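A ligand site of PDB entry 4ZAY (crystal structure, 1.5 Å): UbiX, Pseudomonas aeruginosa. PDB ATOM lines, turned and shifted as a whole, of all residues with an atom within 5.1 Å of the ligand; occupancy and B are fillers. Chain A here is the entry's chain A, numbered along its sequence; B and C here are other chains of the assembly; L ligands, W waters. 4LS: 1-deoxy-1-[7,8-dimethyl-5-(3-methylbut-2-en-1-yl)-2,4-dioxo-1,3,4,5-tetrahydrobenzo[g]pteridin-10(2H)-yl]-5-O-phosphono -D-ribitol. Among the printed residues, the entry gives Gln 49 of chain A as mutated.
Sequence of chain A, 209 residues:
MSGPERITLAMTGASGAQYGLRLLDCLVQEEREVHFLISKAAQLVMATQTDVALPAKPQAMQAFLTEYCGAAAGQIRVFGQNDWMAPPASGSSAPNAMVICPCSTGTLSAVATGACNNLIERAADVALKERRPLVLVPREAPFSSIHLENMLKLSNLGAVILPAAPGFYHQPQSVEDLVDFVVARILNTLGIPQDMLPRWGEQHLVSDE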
ATOM      1  N   THR A  12      25.816  14.084  14.362  1.00  0.00           N
ATOM      2  CA  THR A  12      25.184  13.342  13.276  1.00  0.00           C
ATOM      3  C   THR A  12      23.955  12.601  13.807  1.00  0.00           C
ATOM      4  O   THR A  12      23.700  12.617  14.995  1.00  0.00           O
ATOM      5  CB  THR A  12      26.225  12.445  12.519  1.00  0.00           C
ATOM      6  OG1 THR A  12      26.641  11.403  13.417  1.00  0.00           O
ATOM      7  CG2 THR A  12      27.398  13.250  12.091  1.00  0.00           C
ATOM      8  N   GLY A  13      23.235  11.982  12.905  1.00  0.00           N
ATOM      9  CA  GLY A  13      21.871  11.554  13.105  1.00  0.00           C
ATOM     10  C   GLY A  13      21.606  10.320  13.920  1.00  0.00           C
ATOM     11  O   GLY A  13      20.748   9.564  13.511  1.00  0.00           O
ATOM     12  N   ALA A  14      22.302  10.123  15.030  1.00  0.00           N
ATOM     13  CA  ALA A  14      21.956   9.076  15.972  1.00  0.00           C
ATOM     14  C   ALA A  14      21.119   9.667  17.104  1.00  0.00           C
ATOM     15  O   ALA A  14      21.222  10.835  17.390  1.00  0.00           O
ATOM     16  CB  ALA A  14      23.165   8.374  16.519  1.00  0.00           C
ATOM     17  N   SER A  15      20.258   8.824  17.664  1.00  0.00           N
ATOM     18  CA  SER A  15      19.438   9.179  18.819  1.00  0.00           C
ATOM     19  C   SER A  15      20.087   9.452  20.152  1.00  0.00           C
ATOM     20  O   SER A  15      19.771   8.743  21.131  1.00  0.00           O
ATOM     21  CB  SER A  15      18.371   8.099  18.992  1.00  0.00           C
ATOM     22  OG  SER A  15      17.322   8.510  19.861  1.00  0.00           O
ATOM     23  N   SER A  39      24.687  17.485  10.901  1.00  0.00           N
ATOM     24  CA  SER A  39      24.099  16.980   9.739  1.00  0.00           C
ATOM     25  C   SER A  39      22.573  17.251   9.630  1.00  0.00           C
ATOM     26  O   SER A  39      21.956  17.534  10.623  1.00  0.00           O
ATOM     27  CB  SER A  39      24.348  15.406   9.635  1.00  0.00           C
ATOM     28  OG  SER A  39      23.573  14.749  10.555  1.00  0.00           O
ATOM     29  N   ALA A  41      20.250  14.972   9.142  1.00  0.00           N
ATOM     30  CA  ALA A  41      19.548  14.081   9.979  1.00  0.00           C
ATOM     31  C   ALA A  41      19.670  14.395  11.463  1.00  0.00           C
ATOM     32  O   ALA A  41      18.784  14.178  12.258  1.00  0.00           O
ATOM     33  CB  ALA A  41      20.057  12.624   9.669  1.00  0.00           C
ATOM     34  N   ALA A  42      20.852  14.874  11.916  1.00  0.00           N
ATOM     35  CA  ALA A  42      20.976  15.320  13.285  1.00  0.00           C
ATOM     36  C   ALA A  42      19.994  16.504  13.645  1.00  0.00           C
ATOM     37  O   ALA A  42      19.570  16.549  14.795  1.00  0.00           O
ATOM     38  CB  ALA A  42      22.374  15.727  13.635  1.00  0.00           C
ATOM     39  N   LEU A  44      17.047  16.795  12.499  1.00  0.00           N
ATOM     40  CA  LEU A  44      15.765  16.123  12.755  1.00  0.00           C
ATOM     41  C   LEU A  44      15.757  15.462  14.109  1.00  0.00           C
ATOM     42  O   LEU A  44      14.797  15.538  14.910  1.00  0.00           O
ATOM     43  CB  LEU A  44      15.446  15.134  11.664  1.00  0.00           C
ATOM     44  CG  LEU A  44      15.454  15.656  10.228  1.00  0.00           C
ATOM     45  CD1 LEU A  44      15.422  14.528   9.228  1.00  0.00           C
ATOM     46  CD2 LEU A  44      14.285  16.603   9.984  1.00  0.00           C
ATOM     47  N   VAL A  45      16.857  14.805  14.490  1.00  0.00           N
ATOM     48  CA  VAL A  45      16.899  14.201  15.753  1.00  0.00           C
ATOM     49  C   VAL A  45      16.669  15.265  16.871  1.00  0.00           C
ATOM     50  O   VAL A  45      15.922  15.027  17.827  1.00  0.00           O
ATOM     51  CB  VAL A  45      18.276  13.451  16.009  1.00  0.00           C
ATOM     52  CG1 VAL A  45      18.371  13.015  17.460  1.00  0.00           C
ATOM     53  CG2 VAL A  45      18.405  12.226  15.045  1.00  0.00           C
ATOM     54  N   THR A  48      13.078  16.542  17.174  1.00  0.00           N
ATOM     55  CA  THR A  48      12.141  15.535  17.693  1.00  0.00           C
ATOM     56  C   THR A  48      12.408  14.916  19.021  1.00  0.00           C
ATOM     57  O   THR A  48      11.493  14.335  19.612  1.00  0.00           O
ATOM     58  CB  THR A  48      11.886  14.449  16.641  1.00  0.00           C
ATOM     59  OG1 THR A  48      13.109  13.744  16.360  1.00  0.00           O
ATOM     60  CG2 THR A  48      11.436  15.038  15.338  1.00  0.00           C
ATOM     61  N   GLN A  49      13.613  15.004  19.589  1.00  0.00           N
ATOM     62  CA  GLN A  49      13.964  14.316  20.797  1.00  0.00           C
ATOM     63  C   GLN A  49      14.459  15.228  21.876  1.00  0.00           C
ATOM     64  O   GLN A  49      14.798  14.786  22.933  1.00  0.00           O
ATOM     65  CB  GLN A  49      15.066  13.226  20.509  1.00  0.00           C
ATOM     66  CG  GLN A  49      14.599  12.224  19.508  1.00  0.00           C
ATOM     67  CD  GLN A  49      15.608  11.126  19.234  1.00  0.00           C
ATOM     68  OE1 GLN A  49      16.593  10.968  19.957  1.00  0.00           O
ATOM     69  NE2 GLN A  49      15.306  10.345  18.187  1.00  0.00           N
ATOM     70  N   CYS A 103      27.597   9.772  16.809  1.00  0.00           N
ATOM     71  CA  CYS A 103      28.078   9.332  15.482  1.00  0.00           C
ATOM     72  C   CYS A 103      27.084   8.272  14.926  1.00  0.00           C
ATOM     73  O   CYS A 103      27.029   7.162  15.484  1.00  0.00           O
ATOM     74  CB  CYS A 103      29.410   8.684  15.649  1.00  0.00           C
ATOM     75  SG  CYS A 103      30.137   8.269  13.999  1.00  0.00           S
ATOM     76  N   SER A 104      26.306   8.610  13.916  1.00  0.00           N
ATOM     77  CA  SER A 104      25.428   7.650  13.314  1.00  0.00           C
ATOM     78  C   SER A 104      26.224   6.475  12.697  1.00  0.00           C
ATOM     79  O   SER A 104      27.417   6.610  12.374  1.00  0.00           O
ATOM     80  CB  SER A 104      24.654   8.280  12.163  1.00  0.00           C
ATOM     81  OG  SER A 104      25.481   8.660  11.095  1.00  0.00           O
ATOM     82  N   THR A 105      25.541   5.381  12.410  1.00  0.00           N
ATOM     83  CA  THR A 105      26.207   4.281  11.708  1.00  0.00           C
ATOM     84  C   THR A 105      26.571   4.711  10.314  1.00  0.00           C
ATOM     85  O   THR A 105      27.607   4.254   9.749  1.00  0.00           O
ATOM     86  CB  THR A 105      25.356   3.011  11.695  1.00  0.00           C
ATOM     87  OG1 THR A 105      24.157   3.199  10.954  1.00  0.00           O
ATOM     88  CG2 THR A 105      25.035   2.554  13.087  1.00  0.00           C
ATOM     89  N   GLY A 106      25.816   5.623   9.637  1.00  0.00           N
ATOM     90  CA  GLY A 106      26.209   6.099   8.344  1.00  0.00           C
ATOM     91  C   GLY A 106      27.439   6.921   8.363  1.00  0.00           C
ATOM     92  O   GLY A 106      28.290   6.802   7.431  1.00  0.00           O
ATOM     93  N   THR A 107      27.657   7.804   9.394  1.00  0.00           N
ATOM     94  CA  THR A 107      28.844   8.610   9.446  1.00  0.00           C
ATOM     95  C   THR A 107      30.051   7.690   9.783  1.00  0.00           C
ATOM     96  O   THR A 107      31.169   7.837   9.272  1.00  0.00           O
ATOM     97  CB  THR A 107      28.717   9.815  10.365  1.00  0.00           C
ATOM     98  OG1 THR A 107      27.879  10.771   9.673  1.00  0.00           O
ATOM     99  CG2 THR A 107      30.066  10.430  10.683  1.00  0.00           C
ATOM    100  N   ASN A 118      30.548  15.027   2.795  1.00  0.00           N
ATOM    101  CA  ASN A 118      30.194  16.339   3.391  1.00  0.00           C
ATOM    102  C   ASN A 118      31.318  16.759   4.287  1.00  0.00           C
ATOM    103  O   ASN A 118      32.351  16.045   4.461  1.00  0.00           O
ATOM    104  CB  ASN A 118      28.866  16.226   4.179  1.00  0.00           C
ATOM    105  CG  ASN A 118      28.913  15.137   5.254  1.00  0.00           C
ATOM    106  OD1 ASN A 118      29.845  15.134   6.028  1.00  0.00           O
ATOM    107  ND2 ASN A 118      27.817  14.392   5.411  1.00  0.00           N
ATOM    108  N   ARG A 139      25.768   5.459  18.826  1.00  0.00           N
ATOM    109  CA  ARG A 139      24.595   5.076  19.666  1.00  0.00           C
ATOM    110  C   ARG A 139      23.698   4.266  18.792  1.00  0.00           C
ATOM    111  O   ARG A 139      23.028   4.800  17.920  1.00  0.00           O
ATOM    112  CB  ARG A 139      23.856   6.347  20.155  1.00  0.00           C
ATOM    113  CG  ARG A 139      22.848   6.231  21.290  1.00  0.00           C
ATOM    114  CD  ARG A 139      21.885   5.072  21.261  1.00  0.00           C
ATOM    115  NE  ARG A 139      21.006   4.921  20.075  1.00  0.00           N
ATOM    116  CZ  ARG A 139      20.291   3.842  19.824  1.00  0.00           C
ATOM    117  NH1 ARG A 139      20.253   2.844  20.703  1.00  0.00           N
ATOM    118  NH2 ARG A 139      19.586   3.771  18.723  1.00  0.00           N
ATOM    119  N   GLU A 140      23.794   2.938  18.922  1.00  0.00           N
ATOM    120  CA  GLU A 140      23.020   2.011  18.111  1.00  0.00           C
ATOM    121  C   GLU A 140      22.962   0.728  18.923  1.00  0.00           C
ATOM    122  O   GLU A 140      23.859   0.468  19.736  1.00  0.00           O
ATOM    123  CB  GLU A 140      23.665   1.809  16.724  1.00  0.00           C
ATOM    124  CG  GLU A 140      22.956   0.824  15.782  1.00  0.00           C
ATOM    125  CD  GLU A 140      21.581   1.225  15.513  1.00  0.00           C
ATOM    126  OE1 GLU A 140      20.693   0.957  16.344  1.00  0.00           O
ATOM    127  OE2 GLU A 140      21.290   1.878  14.481  1.00  0.00           O
ATOM    128  N   TRP B  84      12.567   9.181   7.655  1.00  0.00           N
ATOM    129  CA  TRP B  84      13.024   8.496   8.850  1.00  0.00           C
ATOM    130  C   TRP B  84      11.970   8.167   9.854  1.00  0.00           C
ATOM    131  O   TRP B  84      12.190   7.407  10.746  1.00  0.00           O
ATOM    132  CB  TRP B  84      14.171   9.283   9.505  1.00  0.00           C
ATOM    133  CG  TRP B  84      15.224   9.721   8.510  1.00  0.00           C
ATOM    134  CD1 TRP B  84      15.503  10.996   8.113  1.00  0.00           C
ATOM    135  CD2 TRP B  84      16.134   8.877   7.747  1.00  0.00           C
ATOM    136  NE1 TRP B  84      16.496  11.010   7.150  1.00  0.00           N
ATOM    137  CE2 TRP B  84      16.904   9.724   6.943  1.00  0.00           C
ATOM    138  CE3 TRP B  84      16.343   7.498   7.693  1.00  0.00           C
ATOM    139  CZ2 TRP B  84      17.851   9.253   6.041  1.00  0.00           C
ATOM    140  CZ3 TRP B  84      17.317   7.038   6.837  1.00  0.00           C
ATOM    141  CH2 TRP B  84      18.070   7.904   6.036  1.00  0.00           C
ATOM    142  N   ALA B  89      13.327   2.448   9.322  1.00  0.00           N
ATOM    143  CA  ALA B  89      14.442   3.194   9.805  1.00  0.00           C
ATOM    144  C   ALA B  89      14.976   2.774  11.168  1.00  0.00           C
ATOM    145  O   ALA B  89      16.128   3.160  11.539  1.00  0.00           O
ATOM    146  CB  ALA B  89      14.155   4.674   9.820  1.00  0.00           C
ATOM    147  N   SER B  90      14.197   2.005  11.934  1.00  0.00           N
ATOM    148  CA  SER B  90      14.508   1.629  13.274  1.00  0.00           C
ATOM    149  C   SER B  90      14.285   0.154  13.470  1.00  0.00           C
ATOM    150  O   SER B  90      13.287  -0.448  12.938  1.00  0.00           O
ATOM    151  CB  SER B  90      13.616   2.319  14.327  1.00  0.00           C
ATOM    152  OG  SER B  90      13.884   1.835  15.647  1.00  0.00           O
ATOM    153  N   CYS B 116      24.167   3.833   4.623  1.00  0.00           N
ATOM    154  CA  CYS B 116      22.907   4.509   5.173  1.00  0.00           C
ATOM    155  C   CYS B 116      22.651   5.937   4.600  1.00  0.00           C
ATOM    156  O   CYS B 116      22.265   6.851   5.359  1.00  0.00           O
ATOM    157  CB  CYS B 116      22.929   4.550   6.740  1.00  0.00           C
ATOM    158  SG  CYS B 116      22.885   3.044   7.578  1.00  0.00           S
ATOM    159  N   ASN B 117      22.762   6.084   3.279  1.00  0.00           N
ATOM    160  CA  ASN B 117      22.636   7.380   2.584  1.00  0.00           C
ATOM    161  C   ASN B 117      21.134   7.796   2.591  1.00  0.00           C
ATOM    162  O   ASN B 117      20.815   8.962   2.674  1.00  0.00           O
ATOM    163  CB  ASN B 117      23.227   7.348   1.126  1.00  0.00           C
ATOM    164  CG  ASN B 117      24.782   7.088   1.050  1.00  0.00           C
ATOM    165  OD1 ASN B 117      25.571   7.704   1.815  1.00  0.00           O
ATOM    166  ND2 ASN B 117      25.222   6.126   0.143  1.00  0.00           N
ATOM    167  N   ASN B 118      20.236   6.825   2.494  1.00  0.00           N
ATOM    168  CA  ASN B 118      18.783   7.017   2.263  1.00  0.00           C
ATOM    169  C   ASN B 118      18.051   5.923   2.978  1.00  0.00           C
ATOM    170  O   ASN B 118      18.653   5.018   3.631  1.00  0.00           O
ATOM    171  CB  ASN B 118      18.475   6.993   0.746  1.00  0.00           C
ATOM    172  CG  ASN B 118      18.967   5.712   0.068  1.00  0.00           C
ATOM    173  OD1 ASN B 118      18.661   4.648   0.560  1.00  0.00           O
ATOM    174  ND2 ASN B 118      19.517   5.838  -1.142  1.00  0.00           N
ATOM    175  N   ARG B 122      19.504   2.513   4.903  1.00  0.00           N
ATOM    176  CA  ARG B 122      19.300   2.341   6.329  1.00  0.00           C
ATOM    177  C   ARG B 122      18.406   1.183   6.643  1.00  0.00           C
ATOM    178  O   ARG B 122      18.619   0.450   7.617  1.00  0.00           O
ATOM    179  CB  ARG B 122      18.705   3.643   6.895  1.00  0.00           C
ATOM    180  CG  ARG B 122      18.312   3.531   8.364  1.00  0.00           C
ATOM    181  CD  ARG B 122      19.429   3.272   9.350  1.00  0.00           C
ATOM    182  NE  ARG B 122      18.908   3.240  10.718  1.00  0.00           N
ATOM    183  CZ  ARG B 122      19.625   2.923  11.781  1.00  0.00           C
ATOM    184  NH1 ARG B 122      20.917   2.610  11.688  1.00  0.00           N
ATOM    185  NH2 ARG B 122      18.983   2.875  12.939  1.00  0.00           N
ATOM    186  N   TYR C 169      14.663   8.334  21.649  1.00  0.00           N
ATOM    187  CA  TYR C 169      13.500   8.555  20.776  1.00  0.00           C
ATOM    188  C   TYR C 169      12.167   8.262  21.384  1.00  0.00           C
ATOM    189  O   TYR C 169      11.143   8.532  20.728  1.00  0.00           O
ATOM    190  CB  TYR C 169      13.599   7.821  19.472  1.00  0.00           C
ATOM    191  CG  TYR C 169      13.917   6.348  19.497  1.00  0.00           C
ATOM    192  CD1 TYR C 169      12.905   5.336  19.529  1.00  0.00           C
ATOM    193  CD2 TYR C 169      15.247   5.918  19.247  1.00  0.00           C
ATOM    194  CE1 TYR C 169      13.211   3.972  19.351  1.00  0.00           C
ATOM    195  CE2 TYR C 169      15.511   4.564  19.084  1.00  0.00           C
ATOM    196  CZ  TYR C 169      14.518   3.604  19.094  1.00  0.00           C
ATOM    197  OH  TYR C 169      14.811   2.269  18.943  1.00  0.00           O
ATOM    198  N   TRP C 200       8.275   1.420  16.125  1.00  0.00           N
ATOM    199  CA  TRP C 200       8.479   2.585  15.367  1.00  0.00           C
ATOM    200  C   TRP C 200       7.710   2.692  14.073  1.00  0.00           C
ATOM    201  O   TRP C 200       7.743   1.809  13.212  1.00  0.00           O
ATOM    202  CB  TRP C 200       9.981   2.758  15.086  1.00  0.00           C
ATOM    203  CG  TRP C 200      10.326   4.035  14.404  1.00  0.00           C
ATOM    204  CD1 TRP C 200      10.691   4.227  13.097  1.00  0.00           C
ATOM    205  CD2 TRP C 200      10.353   5.329  15.024  1.00  0.00           C
ATOM    206  NE1 TRP C 200      10.927   5.538  12.851  1.00  0.00           N
ATOM    207  CE2 TRP C 200      10.709   6.265  14.018  1.00  0.00           C
ATOM    208  CE3 TRP C 200      10.054   5.797  16.296  1.00  0.00           C
ATOM    209  CZ2 TRP C 200      10.867   7.641  14.276  1.00  0.00           C
ATOM    210  CZ3 TRP C 200      10.210   7.143  16.559  1.00  0.00           C
ATOM    211  CH2 TRP C 200      10.538   8.065  15.554  1.00  0.00           C
HETATM  212  C4A 4LS L   1      19.478   6.502  14.877  1.00  0.00           C
HETATM  213  CAA 4LS L   1      13.589   6.005  15.704  1.00  0.00           C
HETATM  214  CAC 4LS L   1      16.063  10.933  11.789  1.00  0.00           C
HETATM  215  CAD 4LS L   1      14.987  10.597  14.607  1.00  0.00           C
HETATM  216  OAL 4LS L   1      25.283  10.465   9.369  1.00  0.00           O
HETATM  217  PBK 4LS L   1      24.130  11.456   9.029  1.00  0.00           P
HETATM  218  OAM 4LS L   1      24.551  12.426   7.917  1.00  0.00           O
HETATM  219  OAH 4LS L   1      23.554  12.117  10.210  1.00  0.00           O
HETATM  220  OAV 4LS L   1      23.103  10.556   8.290  1.00  0.00           O
HETATM  221  CAR 4LS L   1      22.452   9.481   9.033  1.00  0.00           C
HETATM  222  CBF 4LS L   1      21.285   8.966   8.356  1.00  0.00           C
HETATM  223  OAI 4LS L   1      21.305   8.815   6.989  1.00  0.00           O
HETATM  224  CBH 4LS L   1      20.647   7.888   9.130  1.00  0.00           C
HETATM  225  OAK 4LS L   1      21.000   6.581   8.701  1.00  0.00           O
HETATM  226  CBG 4LS L   1      20.340   8.026  10.504  1.00  0.00           C
HETATM  227  OAJ 4LS L   1      20.116   9.384  10.967  1.00  0.00           O
HETATM  228  CAS 4LS L   1      19.419   7.032  11.170  1.00  0.00           C
HETATM  229  N10 4LS L   1      19.106   7.132  12.583  1.00  0.00           N
HETATM  230  C9A 4LS L   1      18.032   7.980  13.019  1.00  0.00           C
HETATM  231  C9  4LS L   1      17.526   9.004  12.193  1.00  0.00           C
HETATM  232  C8  4LS L   1      16.527   9.879  12.724  1.00  0.00           C
HETATM  233  C7  4LS L   1      16.092   9.699  14.003  1.00  0.00           C
HETATM  234  C6  4LS L   1      16.602   8.711  14.838  1.00  0.00           C
HETATM  235  C5A 4LS L   1      17.646   7.858  14.315  1.00  0.00           C
HETATM  236  N5  4LS L   1      18.102   6.911  15.225  1.00  0.00           N
HETATM  237  CAQ 4LS L   1      17.371   5.587  15.004  1.00  0.00           C
HETATM  238  CAN 4LS L   1      16.024   5.629  15.580  1.00  0.00           C
HETATM  239  CAW 4LS L   1      14.799   5.871  14.836  1.00  0.00           C
HETATM  240  CAB 4LS L   1      14.660   6.041  13.344  1.00  0.00           C
HETATM  241  C11 4LS L   1      19.835   6.558  13.541  1.00  0.00           C
HETATM  242  N1  4LS L   1      21.131   6.133  13.224  1.00  0.00           N
HETATM  243  C2  4LS L   1      21.904   5.599  14.176  1.00  0.00           C
HETATM  244  O2  4LS L   1      23.133   5.243  13.885  1.00  0.00           O
HETATM  245  N3  4LS L   1      21.548   5.569  15.493  1.00  0.00           N
HETATM  246  C4  4LS L   1      20.241   6.009  15.913  1.00  0.00           C
HETATM  247  O4  4LS L   1      20.048   6.013  17.151  1.00  0.00           O
HETATM  248  O   HOH W   1      22.275  13.897   7.216  1.00  0.00           O
HETATM  249  O   HOH W   2      24.805  12.039   5.338  1.00  0.00           O
HETATM  250  O   HOH W   3      27.259  13.323   8.064  1.00  0.00           O
HETATM  251  O   HOH W   4      25.414   5.041  15.908  1.00  0.00           O
HETATM  252  O   HOH W   5      22.728   5.597  10.756  1.00  0.00           O
HETATM  253  O   HOH W   6      26.058   9.329   6.953  1.00  0.00           O
HETATM  254  O   HOH W   7      12.673  10.986  16.910  1.00  0.00           O
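An oxygen (OAL) of the ligand sits at hydrogen-bond distance from the side-chain hydroxyl (OG) of Ser 104.
An oxygen (OAH) of the ligand lies within hydrogen-bond range of the backbone NH (N) of Gly 13, 2.7 Å away.
O of Gly 13 is in hydrogen-bond range of OAJ of the ligand (2.6 Å).
The side-chain hydroxyl (OG1) of Thr 107 is in hydrogen-bond range of an oxygen (OAL) of the ligand (2.6 Å).
OG of Ser 39 sits at hydrogen-bond distance from OAH of the ligand.
OAI of the ligand sits at hydrogen-bond distance from O of Cys 116 of chain B (2.7 Å).
O of Arg 139 lies within hydrogen-bond range of N3 of the ligand (2.9 Å).
NH2 of Arg 139 lies within hydrogen-bond range of O4 of the ligand (2.8 Å).
N of Thr 105 lies within hydrogen-bond range of O2 of the ligand (2.8 Å).
N of Ser 15 is in hydrogen-bond range of O4 of the ligand, 2.9 Å away.
The backbone NH (N) of Thr 107 is in hydrogen-bond range of the side-chain hydroxyl (OG) of Ser 104 (2.9 Å).
The side-chain hydroxyl (OG) of Ser 104 sits close to the backbone NH (N) of Gly 106 (3.4 Å).
The side-chain sulfur (SG) of Cys 116 of chain B sits at hydrogen-bond distance from the side-chain hydroxyl (OG1) of Thr 105 (3.6 Å).
The side-chain hydroxyl (OG1) of Thr 105 is in hydrogen-bond range of the guanidinium group (NH1) of Arg 122 of chain B (3.4 Å).
The indole nitrogen (NE1) of Trp 200 of chain C is in hydrogen-bond range of the backbone carbonyl oxygen (O) of Trp 84 of chain B, at 3.1 Å.
The backbone carbonyl oxygen of Val 45 lies within hydrogen-bond range of the side-chain hydroxyl of Thr 48.
OH of Tyr 169 of chain C is in hydrogen-bond range of OG of Ser 90 of chain B, at 3.5 Å.
The backbone carbonyl oxygen (O) of Ala 89 of chain B sits at hydrogen-bond distance from the guanidinium group (NE) of Arg 122 of chain B (2.9 Å).
Residues that only touch the ligand: Trp 200 of chain C, Trp 84 of chain B, Ala 14, Ala 41, Thr 12, Val 45, Gln 49, Tyr 169 of chain C, Ala 89 of chain B, Arg 122 of chain B, Ser 90 of chain B and Glu 140.
Hydrophobic or aromatic side chains that line the ligand: Ala 14, Ala 41, Val 45, Trp 84 of chain B, Ala 89 of chain B, Tyr 169 of chain C and Trp 200 of chain C.
Within 4 Å of the ligand: Thr 12, Gly 13, Ala 14, Ser 15, Ser 39, Ala 41, Val 45, Gln 49, Ser 104, Thr 105, Thr 107, Arg 139, Glu 140, Trp 84 of chain B, Ala 89 of chain B, Ser 90 of chain B, Cys 116 of chain B, Arg 122 of chain B, Tyr 169 of chain C and Trp 200 of chain C.
Along chain A the residues within 4 Å of the ligand span positions 12 to 140.
The nearest printed residue that does not touch the ligand is Thr 48 (4.1 Å).
Water W6 lies within hydrogen-bond range of an oxygen (OAL) of the ligand (2.8 Å), the backbone NH of Thr 107 (3.3 Å) and the backbone carbonyl oxygen of Gly 106 (3.4 Å).
Water W1 lies within hydrogen-bond range of OAM of the ligand and N of Ala 41.
Water W3 lies within hydrogen-bond range of OAM of the ligand, ND2 of Asn 118 of chain A and OG1 of Thr 107.
Water W5 lies within hydrogen-bond range of OG1 of Thr 105 (2.8 Å), OAK of the ligand (2.9 Å) and N of Gly 106 (3.3 Å).
Water W4 lies within hydrogen-bond range of the backbone carbonyl oxygen of Cys 103, the backbone NH of Arg 139 and an oxygen (O2) of the ligand.
Water W7 bridges the side-chain hydroxyl (OG1) of Thr 48 and the side-chain amide nitrogen (NE2) of Gln 49.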
